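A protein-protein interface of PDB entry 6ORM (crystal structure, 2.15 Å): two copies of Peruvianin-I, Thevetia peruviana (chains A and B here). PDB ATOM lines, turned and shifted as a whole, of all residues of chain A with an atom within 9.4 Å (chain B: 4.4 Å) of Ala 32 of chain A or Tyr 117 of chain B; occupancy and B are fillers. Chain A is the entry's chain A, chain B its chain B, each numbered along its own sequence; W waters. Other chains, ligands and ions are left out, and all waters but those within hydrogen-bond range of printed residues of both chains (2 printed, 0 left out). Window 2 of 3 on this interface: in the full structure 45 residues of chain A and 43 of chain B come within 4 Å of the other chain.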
ATOM      1  N   ASP A   9       7.464  -1.304 -19.679  1.00  0.00           N
ATOM      2  CA  ASP A   9       6.841  -1.046 -20.977  1.00  0.00           C
ATOM      3  C   ASP A   9       7.354   0.250 -21.589  1.00  0.00           C
ATOM      4  O   ASP A   9       7.822   0.273 -22.733  1.00  0.00           O
ATOM      5  CB  ASP A   9       5.321  -0.986 -20.832  1.00  0.00           C
ATOM      6  CG  ASP A   9       4.710  -2.328 -20.509  1.00  0.00           C
ATOM      7  OD1 ASP A   9       5.445  -3.336 -20.472  1.00  0.00           O
ATOM      8  OD2 ASP A   9       3.480  -2.373 -20.294  1.00  0.00           O
ATOM      9  N   PHE A  10       7.288   1.341 -20.832  1.00  0.00           N
ATOM     10  CA  PHE A  10       7.747   2.633 -21.316  1.00  0.00           C
ATOM     11  C   PHE A  10       8.183   3.464 -20.121  1.00  0.00           C
ATOM     12  O   PHE A  10       7.956   3.098 -18.964  1.00  0.00           O
ATOM     13  CB  PHE A  10       6.667   3.353 -22.136  1.00  0.00           C
ATOM     14  CG  PHE A  10       5.337   3.432 -21.453  1.00  0.00           C
ATOM     15  CD1 PHE A  10       5.095   4.398 -20.489  1.00  0.00           C
ATOM     16  CD2 PHE A  10       4.326   2.543 -21.776  1.00  0.00           C
ATOM     17  CE1 PHE A  10       3.873   4.472 -19.859  1.00  0.00           C
ATOM     18  CE2 PHE A  10       3.098   2.612 -21.149  1.00  0.00           C
ATOM     19  CZ  PHE A  10       2.870   3.578 -20.188  1.00  0.00           C
ATOM     20  N   CYS A  11       8.807   4.598 -20.421  1.00  0.00           N
ATOM     21  CA  CYS A  11       9.465   5.412 -19.410  1.00  0.00           C
ATOM     22  C   CYS A  11       9.690   6.805 -19.980  1.00  0.00           C
ATOM     23  O   CYS A  11      10.806   7.133 -20.394  1.00  0.00           O
ATOM     24  CB  CYS A  11      10.790   4.764 -18.993  1.00  0.00           C
ATOM     25  SG  CYS A  11      11.509   5.357 -17.449  1.00  0.00           S
ATOM     26  N   LEU A  12       8.635   7.620 -20.028  1.00  0.00           N
ATOM     27  CA  LEU A  12       8.713   8.894 -20.732  1.00  0.00           C
ATOM     28  C   LEU A  12       9.733   9.803 -20.066  1.00  0.00           C
ATOM     29  O   LEU A  12       9.690  10.018 -18.853  1.00  0.00           O
ATOM     30  CB  LEU A  12       7.349   9.582 -20.750  1.00  0.00           C
ATOM     31  CG  LEU A  12       6.105   8.763 -21.084  1.00  0.00           C
ATOM     32  CD1 LEU A  12       4.889   9.669 -21.053  1.00  0.00           C
ATOM     33  CD2 LEU A  12       6.244   8.093 -22.434  1.00  0.00           C
ATOM     34  N   ALA A  13      10.651  10.334 -20.870  1.00  0.00           N
ATOM     35  CA  ALA A  13      11.671  11.235 -20.355  1.00  0.00           C
ATOM     36  C   ALA A  13      11.034  12.412 -19.626  1.00  0.00           C
ATOM     37  O   ALA A  13      10.178  13.112 -20.175  1.00  0.00           O
ATOM     38  CB  ALA A  13      12.561  11.734 -21.496  1.00  0.00           C
ATOM     39  N   ARG A  27       8.869  10.237 -16.118  1.00  0.00           N
ATOM     40  CA  ARG A  27       7.610  10.586 -15.488  1.00  0.00           C
ATOM     41  C   ARG A  27       6.894   9.321 -15.032  1.00  0.00           C
ATOM     42  O   ARG A  27       7.194   8.210 -15.480  1.00  0.00           O
ATOM     43  CB  ARG A  27       6.740  11.396 -16.442  1.00  0.00           C
ATOM     44  CG  ARG A  27       7.434  12.646 -16.942  1.00  0.00           C
ATOM     45  CD  ARG A  27       6.532  13.460 -17.835  1.00  0.00           C
ATOM     46  NE  ARG A  27       7.186  13.778 -19.098  1.00  0.00           N
ATOM     47  CZ  ARG A  27       6.572  13.761 -20.274  1.00  0.00           C
ATOM     48  NH1 ARG A  27       5.286  13.450 -20.348  1.00  0.00           N
ATOM     49  NH2 ARG A  27       7.242  14.061 -21.373  1.00  0.00           N
ATOM     50  N   ASN A  28       5.937   9.500 -14.131  1.00  0.00           N
ATOM     51  CA  ASN A  28       5.113   8.408 -13.631  1.00  0.00           C
ATOM     52  C   ASN A  28       4.382   7.734 -14.787  1.00  0.00           C
ATOM     53  O   ASN A  28       3.508   8.350 -15.408  1.00  0.00           O
ATOM     54  CB  ASN A  28       4.122   8.939 -12.593  1.00  0.00           C
ATOM     55  CG  ASN A  28       3.318   7.841 -11.921  1.00  0.00           C
ATOM     56  OD1 ASN A  28       3.338   6.683 -12.340  1.00  0.00           O
ATOM     57  ND2 ASN A  28       2.610   8.204 -10.859  1.00  0.00           N
ATOM     58  N   PRO A  29       4.702   6.471 -15.094  1.00  0.00           N
ATOM     59  CA  PRO A  29       4.060   5.807 -16.242  1.00  0.00           C
ATOM     60  C   PRO A  29       2.550   5.725 -16.126  1.00  0.00           C
ATOM     61  O   PRO A  29       1.869   5.634 -17.155  1.00  0.00           O
ATOM     62  CB  PRO A  29       4.696   4.409 -16.253  1.00  0.00           C
ATOM     63  CG  PRO A  29       5.891   4.495 -15.363  1.00  0.00           C
ATOM     64  CD  PRO A  29       5.637   5.586 -14.379  1.00  0.00           C
ATOM     65  N   ALA A  30       2.004   5.762 -14.907  1.00  0.00           N
ATOM     66  CA  ALA A  30       0.558   5.760 -14.733  1.00  0.00           C
ATOM     67  C   ALA A  30      -0.085   7.023 -15.288  1.00  0.00           C
ATOM     68  O   ALA A  30      -1.292   7.024 -15.553  1.00  0.00           O
ATOM     69  CB  ALA A  30       0.205   5.598 -13.253  1.00  0.00           C
ATOM     70  N   LEU A  31       0.692   8.089 -15.470  1.00  0.00           N
ATOM     71  CA  LEU A  31       0.188   9.346 -16.003  1.00  0.00           C
ATOM     72  C   LEU A  31       0.283   9.431 -17.519  1.00  0.00           C
ATOM     73  O   LEU A  31      -0.238  10.389 -18.101  1.00  0.00           O
ATOM     74  CB  LEU A  31       0.940  10.525 -15.378  1.00  0.00           C
ATOM     75  CG  LEU A  31       0.812  10.634 -13.857  1.00  0.00           C
ATOM     76  CD1 LEU A  31       1.529  11.872 -13.340  1.00  0.00           C
ATOM     77  CD2 LEU A  31      -0.654  10.640 -13.443  1.00  0.00           C
ATOM     78  N   ALA A  32       0.941   8.472 -18.166  1.00  0.00           N
ATOM     79  CA  ALA A  32       1.058   8.488 -19.618  1.00  0.00           C
ATOM     80  C   ALA A  32      -0.310   8.343 -20.277  1.00  0.00           C
ATOM     81  O   ALA A  32      -1.186   7.626 -19.786  1.00  0.00           O
ATOM     82  CB  ALA A  32       1.987   7.369 -20.086  1.00  0.00           C
ATOM     83  N   THR A  33      -0.493   9.046 -21.392  1.00  0.00           N
ATOM     84  CA  THR A  33      -1.706   8.965 -22.195  1.00  0.00           C
ATOM     85  C   THR A  33      -1.325   8.689 -23.644  1.00  0.00           C
ATOM     86  O   THR A  33      -0.146   8.670 -24.006  1.00  0.00           O
ATOM     87  CB  THR A  33      -2.543  10.251 -22.102  1.00  0.00           C
ATOM     88  OG1 THR A  33      -1.855  11.319 -22.765  1.00  0.00           O
ATOM     89  CG2 THR A  33      -2.792  10.634 -20.647  1.00  0.00           C
ATOM     90  N   SER A  34      -2.348   8.455 -24.474  1.00  0.00           N
ATOM     91  CA  SER A  34      -2.119   8.202 -25.895  1.00  0.00           C
ATOM     92  C   SER A  34      -1.300   9.310 -26.549  1.00  0.00           C
ATOM     93  O   SER A  34      -0.450   9.039 -27.406  1.00  0.00           O
ATOM     94  CB  SER A  34      -3.454   8.028 -26.619  1.00  0.00           C
ATOM     95  OG  SER A  34      -4.157   6.905 -26.120  1.00  0.00           O
ATOM     96  N   ASP A  35      -1.542  10.566 -26.156  1.00  0.00           N
ATOM     97  CA  ASP A  35      -0.847  11.694 -26.771  1.00  0.00           C
ATOM     98  C   ASP A  35       0.660  11.633 -26.572  1.00  0.00           C
ATOM     99  O   ASP A  35       1.402  12.235 -27.354  1.00  0.00           O
ATOM    100  CB  ASP A  35      -1.366  13.017 -26.200  1.00  0.00           C
ATOM    101  CG  ASP A  35      -2.766  13.351 -26.667  1.00  0.00           C
ATOM    102  OD1 ASP A  35      -3.121  12.970 -27.800  1.00  0.00           O
ATOM    103  OD2 ASP A  35      -3.508  14.014 -25.909  1.00  0.00           O
ATOM    104  N   ASP A  36       1.130  10.916 -25.550  1.00  0.00           N
ATOM    105  CA  ASP A  36       2.557  10.851 -25.266  1.00  0.00           C
ATOM    106  C   ASP A  36       3.323   9.976 -26.246  1.00  0.00           C
ATOM    107  O   ASP A  36       4.557  10.028 -26.260  1.00  0.00           O
ATOM    108  CB  ASP A  36       2.780  10.335 -23.845  1.00  0.00           C
ATOM    109  CG  ASP A  36       2.322  11.319 -22.791  1.00  0.00           C
ATOM    110  OD1 ASP A  36       2.716  12.501 -22.867  1.00  0.00           O
ATOM    111  OD2 ASP A  36       1.562  10.911 -21.886  1.00  0.00           O
ATOM    112  N   PHE A  37       2.638   9.192 -27.072  1.00  0.00           N
ATOM    113  CA  PHE A  37       3.303   8.238 -27.946  1.00  0.00           C
ATOM    114  C   PHE A  37       3.253   8.648 -29.408  1.00  0.00           C
ATOM    115  O   PHE A  37       3.726   7.900 -30.270  1.00  0.00           O
ATOM    116  CB  PHE A  37       2.701   6.847 -27.731  1.00  0.00           C
ATOM    117  CG  PHE A  37       2.891   6.336 -26.329  1.00  0.00           C
ATOM    118  CD1 PHE A  37       4.064   5.699 -25.966  1.00  0.00           C
ATOM    119  CD2 PHE A  37       1.916   6.536 -25.363  1.00  0.00           C
ATOM    120  CE1 PHE A  37       4.256   5.246 -24.675  1.00  0.00           C
ATOM    121  CE2 PHE A  37       2.101   6.084 -24.067  1.00  0.00           C
ATOM    122  CZ  PHE A  37       3.275   5.437 -23.724  1.00  0.00           C
ATOM    123  N   ILE A  38       2.697   9.817 -29.704  1.00  0.00           N
ATOM    124  CA  ILE A  38       2.755  10.420 -31.027  1.00  0.00           C
ATOM    125  C   ILE A  38       3.724  11.596 -30.970  1.00  0.00           C
ATOM    126  O   ILE A  38       3.854  12.267 -29.940  1.00  0.00           O
ATOM    127  CB  ILE A  38       1.354  10.864 -31.501  1.00  0.00           C
ATOM    128  CG1 ILE A  38       1.389  11.351 -32.953  1.00  0.00           C
ATOM    129  CG2 ILE A  38       0.790  11.937 -30.584  1.00  0.00           C
ATOM    130  CD1 ILE A  38       0.035  11.779 -33.483  1.00  0.00           C
ATOM    131  N   PRO A  65       9.771  12.430 -25.745  1.00  0.00           N
ATOM    132  CA  PRO A  65      10.044  11.742 -24.467  1.00  0.00           C
ATOM    133  C   PRO A  65       9.735  10.253 -24.462  1.00  0.00           C
ATOM    134  O   PRO A  65      10.398   9.500 -23.735  1.00  0.00           O
ATOM    135  CB  PRO A  65       9.154  12.503 -23.476  1.00  0.00           C
ATOM    136  CG  PRO A  65       9.016  13.866 -24.068  1.00  0.00           C
ATOM    137  CD  PRO A  65       9.011  13.679 -25.558  1.00  0.00           C
ATOM    138  N   ALA A  66       8.761   9.797 -25.251  1.00  0.00           N
ATOM    139  CA  ALA A  66       8.424   8.379 -25.269  1.00  0.00           C
ATOM    140  C   ALA A  66       9.539   7.509 -25.837  1.00  0.00           C
ATOM    141  O   ALA A  66       9.497   6.288 -25.654  1.00  0.00           O
ATOM    142  CB  ALA A  66       7.137   8.152 -26.064  1.00  0.00           C
ATOM    143  N   GLU B 106      -3.200   4.110 -35.123  1.00  0.00           N
ATOM    144  CA  GLU B 106      -2.091   3.299 -34.641  1.00  0.00           C
ATOM    145  C   GLU B 106      -2.206   3.182 -33.130  1.00  0.00           C
ATOM    146  O   GLU B 106      -2.347   4.195 -32.437  1.00  0.00           O
ATOM    147  CB  GLU B 106      -0.744   3.910 -35.028  1.00  0.00           C
ATOM    148  CG  GLU B 106       0.458   3.089 -34.592  1.00  0.00           C
ATOM    149  CD  GLU B 106       0.741   1.925 -35.521  1.00  0.00           C
ATOM    150  OE1 GLU B 106       0.446   2.041 -36.729  1.00  0.00           O
ATOM    151  OE2 GLU B 106       1.262   0.894 -35.042  1.00  0.00           O
ATOM    152  N   GLY B 107      -2.153   1.955 -32.619  1.00  0.00           N
ATOM    153  CA  GLY B 107      -2.226   1.753 -31.184  1.00  0.00           C
ATOM    154  C   GLY B 107      -1.454   0.532 -30.739  1.00  0.00           C
ATOM    155  O   GLY B 107      -1.225  -0.402 -31.514  1.00  0.00           O
ATOM    156  N   PHE B 108      -1.053   0.553 -29.467  1.00  0.00           N
ATOM    157  CA  PHE B 108      -0.448  -0.601 -28.818  1.00  0.00           C
ATOM    158  C   PHE B 108      -1.046  -0.769 -27.428  1.00  0.00           C
ATOM    159  O   PHE B 108      -1.573   0.177 -26.836  1.00  0.00           O
ATOM    160  CB  PHE B 108       1.087  -0.481 -28.754  1.00  0.00           C
ATOM    161  CG  PHE B 108       1.593   0.430 -27.664  1.00  0.00           C
ATOM    162  CD1 PHE B 108       1.865  -0.062 -26.394  1.00  0.00           C
ATOM    163  CD2 PHE B 108       1.820   1.772 -27.919  1.00  0.00           C
ATOM    164  CE1 PHE B 108       2.332   0.773 -25.397  1.00  0.00           C
ATOM    165  CE2 PHE B 108       2.291   2.611 -26.928  1.00  0.00           C
ATOM    166  CZ  PHE B 108       2.546   2.111 -25.665  1.00  0.00           C
ATOM    167  N   SER B 110      -0.341  -1.988 -23.450  1.00  0.00           N
ATOM    168  CA  SER B 110       0.676  -2.199 -22.435  1.00  0.00           C
ATOM    169  C   SER B 110       0.467  -3.541 -21.734  1.00  0.00           C
ATOM    170  O   SER B 110      -0.535  -4.234 -21.935  1.00  0.00           O
ATOM    171  CB  SER B 110       0.656  -1.060 -21.415  1.00  0.00           C
ATOM    172  OG  SER B 110      -0.370  -1.249 -20.455  1.00  0.00           O
ATOM    173  N   GLN B 115      -3.889  -1.766 -21.206  1.00  0.00           N
ATOM    174  CA  GLN B 115      -4.292  -0.393 -21.471  1.00  0.00           C
ATOM    175  C   GLN B 115      -3.913  -0.021 -22.898  1.00  0.00           C
ATOM    176  O   GLN B 115      -2.795  -0.288 -23.347  1.00  0.00           O
ATOM    177  CB  GLN B 115      -3.643   0.573 -20.481  1.00  0.00           C
ATOM    178  CG  GLN B 115      -3.961   2.034 -20.792  1.00  0.00           C
ATOM    179  CD  GLN B 115      -3.790   2.951 -19.596  1.00  0.00           C
ATOM    180  OE1 GLN B 115      -3.488   2.501 -18.490  1.00  0.00           O
ATOM    181  NE2 GLN B 115      -3.992   4.249 -19.812  1.00  0.00           N
ATOM    182  N   LEU B 116      -4.856   0.579 -23.614  1.00  0.00           N
ATOM    183  CA  LEU B 116      -4.688   0.873 -25.027  1.00  0.00           C
ATOM    184  C   LEU B 116      -4.282   2.328 -25.210  1.00  0.00           C
ATOM    185  O   LEU B 116      -4.971   3.237 -24.730  1.00  0.00           O
ATOM    186  CB  LEU B 116      -5.976   0.574 -25.796  1.00  0.00           C
ATOM    187  CG  LEU B 116      -6.006   0.989 -27.267  1.00  0.00           C
ATOM    188  CD1 LEU B 116      -4.904   0.291 -28.052  1.00  0.00           C
ATOM    189  CD2 LEU B 116      -7.368   0.683 -27.865  1.00  0.00           C
ATOM    190  N   TYR B 117      -3.164   2.540 -25.901  1.00  0.00           N
ATOM    191  CA  TYR B 117      -2.698   3.862 -26.304  1.00  0.00           C
ATOM    192  C   TYR B 117      -2.802   3.933 -27.820  1.00  0.00           C
ATOM    193  O   TYR B 117      -2.070   3.235 -28.527  1.00  0.00           O
ATOM    194  CB  TYR B 117      -1.264   4.112 -25.839  1.00  0.00           C
ATOM    195  CG  TYR B 117      -1.073   3.933 -24.355  1.00  0.00           C
ATOM    196  CD1 TYR B 117      -0.819   2.680 -23.816  1.00  0.00           C
ATOM    197  CD2 TYR B 117      -1.164   5.014 -23.488  1.00  0.00           C
ATOM    198  CE1 TYR B 117      -0.653   2.507 -22.459  1.00  0.00           C
ATOM    199  CE2 TYR B 117      -0.999   4.850 -22.125  1.00  0.00           C
ATOM    200  CZ  TYR B 117      -0.744   3.594 -21.618  1.00  0.00           C
ATOM    201  OH  TYR B 117      -0.576   3.420 -20.265  1.00  0.00           O
ATOM    202  N   VAL B 118      -3.709   4.768 -28.318  1.00  0.00           N
ATOM    203  CA  VAL B 118      -4.044   4.796 -29.736  1.00  0.00           C
ATOM    204  C   VAL B 118      -4.149   6.248 -30.178  1.00  0.00           C
ATOM    205  O   VAL B 118      -4.681   7.094 -29.452  1.00  0.00           O
ATOM    206  CB  VAL B 118      -5.347   4.016 -30.025  1.00  0.00           C
ATOM    207  CG1 VAL B 118      -6.501   4.548 -29.181  1.00  0.00           C
ATOM    208  CG2 VAL B 118      -5.688   4.051 -31.514  1.00  0.00           C
ATOM    209  N   PHE B 127       5.021   7.441 -34.282  1.00  0.00           N
ATOM    210  CA  PHE B 127       4.396   6.720 -33.182  1.00  0.00           C
ATOM    211  C   PHE B 127       5.326   5.585 -32.785  1.00  0.00           C
ATOM    212  O   PHE B 127       5.783   4.829 -33.646  1.00  0.00           O
ATOM    213  CB  PHE B 127       3.019   6.187 -33.592  1.00  0.00           C
ATOM    214  CG  PHE B 127       2.174   5.721 -32.441  1.00  0.00           C
ATOM    215  CD1 PHE B 127       2.268   4.420 -31.979  1.00  0.00           C
ATOM    216  CD2 PHE B 127       1.278   6.582 -31.826  1.00  0.00           C
ATOM    217  CE1 PHE B 127       1.487   3.982 -30.926  1.00  0.00           C
ATOM    218  CE2 PHE B 127       0.494   6.153 -30.770  1.00  0.00           C
ATOM    219  CZ  PHE B 127       0.599   4.850 -30.319  1.00  0.00           C
HETATM  220  O   HOH W   1      -0.701   5.154 -18.505  1.00  0.00           O
HETATM  221  O   HOH W   2      -2.807   4.384 -16.749  1.00  0.00           O
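The backbone NH of Val 118 of chain B sits at hydrogen-bond distance from the side-chain hydroxyl of Ser 34 of chain A (3.1 Å).
N of Ser 110 of chain B is in hydrogen-bond range of O of Gln 115 of chain B.
N of Asp 35 of chain A lies close to OG1 of Thr 33 of chain A (3.5 Å).
The side-chain carboxylate (OD2) of Asp 36 of chain A lies within hydrogen-bond range of the backbone NH (N) of Thr 33 of chain A (2.8 Å).
The backbone NH of Tyr 117 of chain B lies within hydrogen-bond range of the backbone carbonyl oxygen of Phe 108 of chain B.
Among the printed residues, merely in contact across the chains: Asp 9 of chain A with Ser 110 of chain B, Phe 10 of chain A with Tyr 117 of chain B, Ala 32 of chain A with Tyr 117 of chain B, Thr 33 of chain A with Tyr 117 of chain B, Ser 34 of chain A with Tyr 117 of chain B, Phe 37 of chain A with Phe 108 of chain B, Phe 37 of chain A with Tyr 117 of chain B and Phe 37 of chain A with Phe 127 of chain B.
Of the printed residues of chain B, Asp 9 of chain A touches Ser 110.
Leu 31 of chain A touches none of the printed residues of chain B.
Ala 32 of chain A touches just one residue of chain B: Tyr 117 (3.6 Å).
Of the printed residues of chain B, Ser 34 of chain A touches Tyr 117 and Val 118.
Of chain A, only Phe 37 (3.7 Å) comes within 4 Å of Phe 108 of chain B.
Of the printed residues of chain A, Ser 110 of chain B touches Asp 9 (3.3 Å).
Of chain A, only Phe 10 (3.5 Å), Ala 32 (3.6 Å), Thr 33 (3.7 Å), Ser 34 (3.4 Å) and Phe 37 (3.5 Å) come within 4 Å of Tyr 117 of chain B.
Of chain A, only Ser 34 comes within 4 Å of Val 118 of chain B.
Printed residues of chain A within 4 Å of Phe 127 of chain B: Phe 37.
The nearest residue of chain A that does not touch Tyr 117 of chain B is Pro 29 of chain A (4.5 Å).
Of the 19 printed residues of chain A, 6 touch a printed residue of chain B.
Hydrophobic or aromatic side chains of chain A within 4 Å of the printed part of chain B: Phe 10 and Phe 37.
Hydrophobic or aromatic side chains of chain B that line the printed part of chain A: Phe 108, Tyr 117 and Phe 127.
Among the printed residues, 9 pairs touch across the chains.
Among the printed residues, no Asp or Glu carboxylate lies within 4 Å of a Lys or Arg side-chain nitrogen of the other chain.
No position is printed for both chains.
Water W1 lies within hydrogen-bond range of the side-chain hydroxyl of Tyr 117 of chain B, the backbone carbonyl oxygen of Ala 32 of chain A and the backbone carbonyl oxygen of Pro 29 of chain A.
Water W2 lies within hydrogen-bond range of OE1 of Gln 115 of chain B (2.7 Å) and O of Ala 30 of chain A (3.3 Å).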
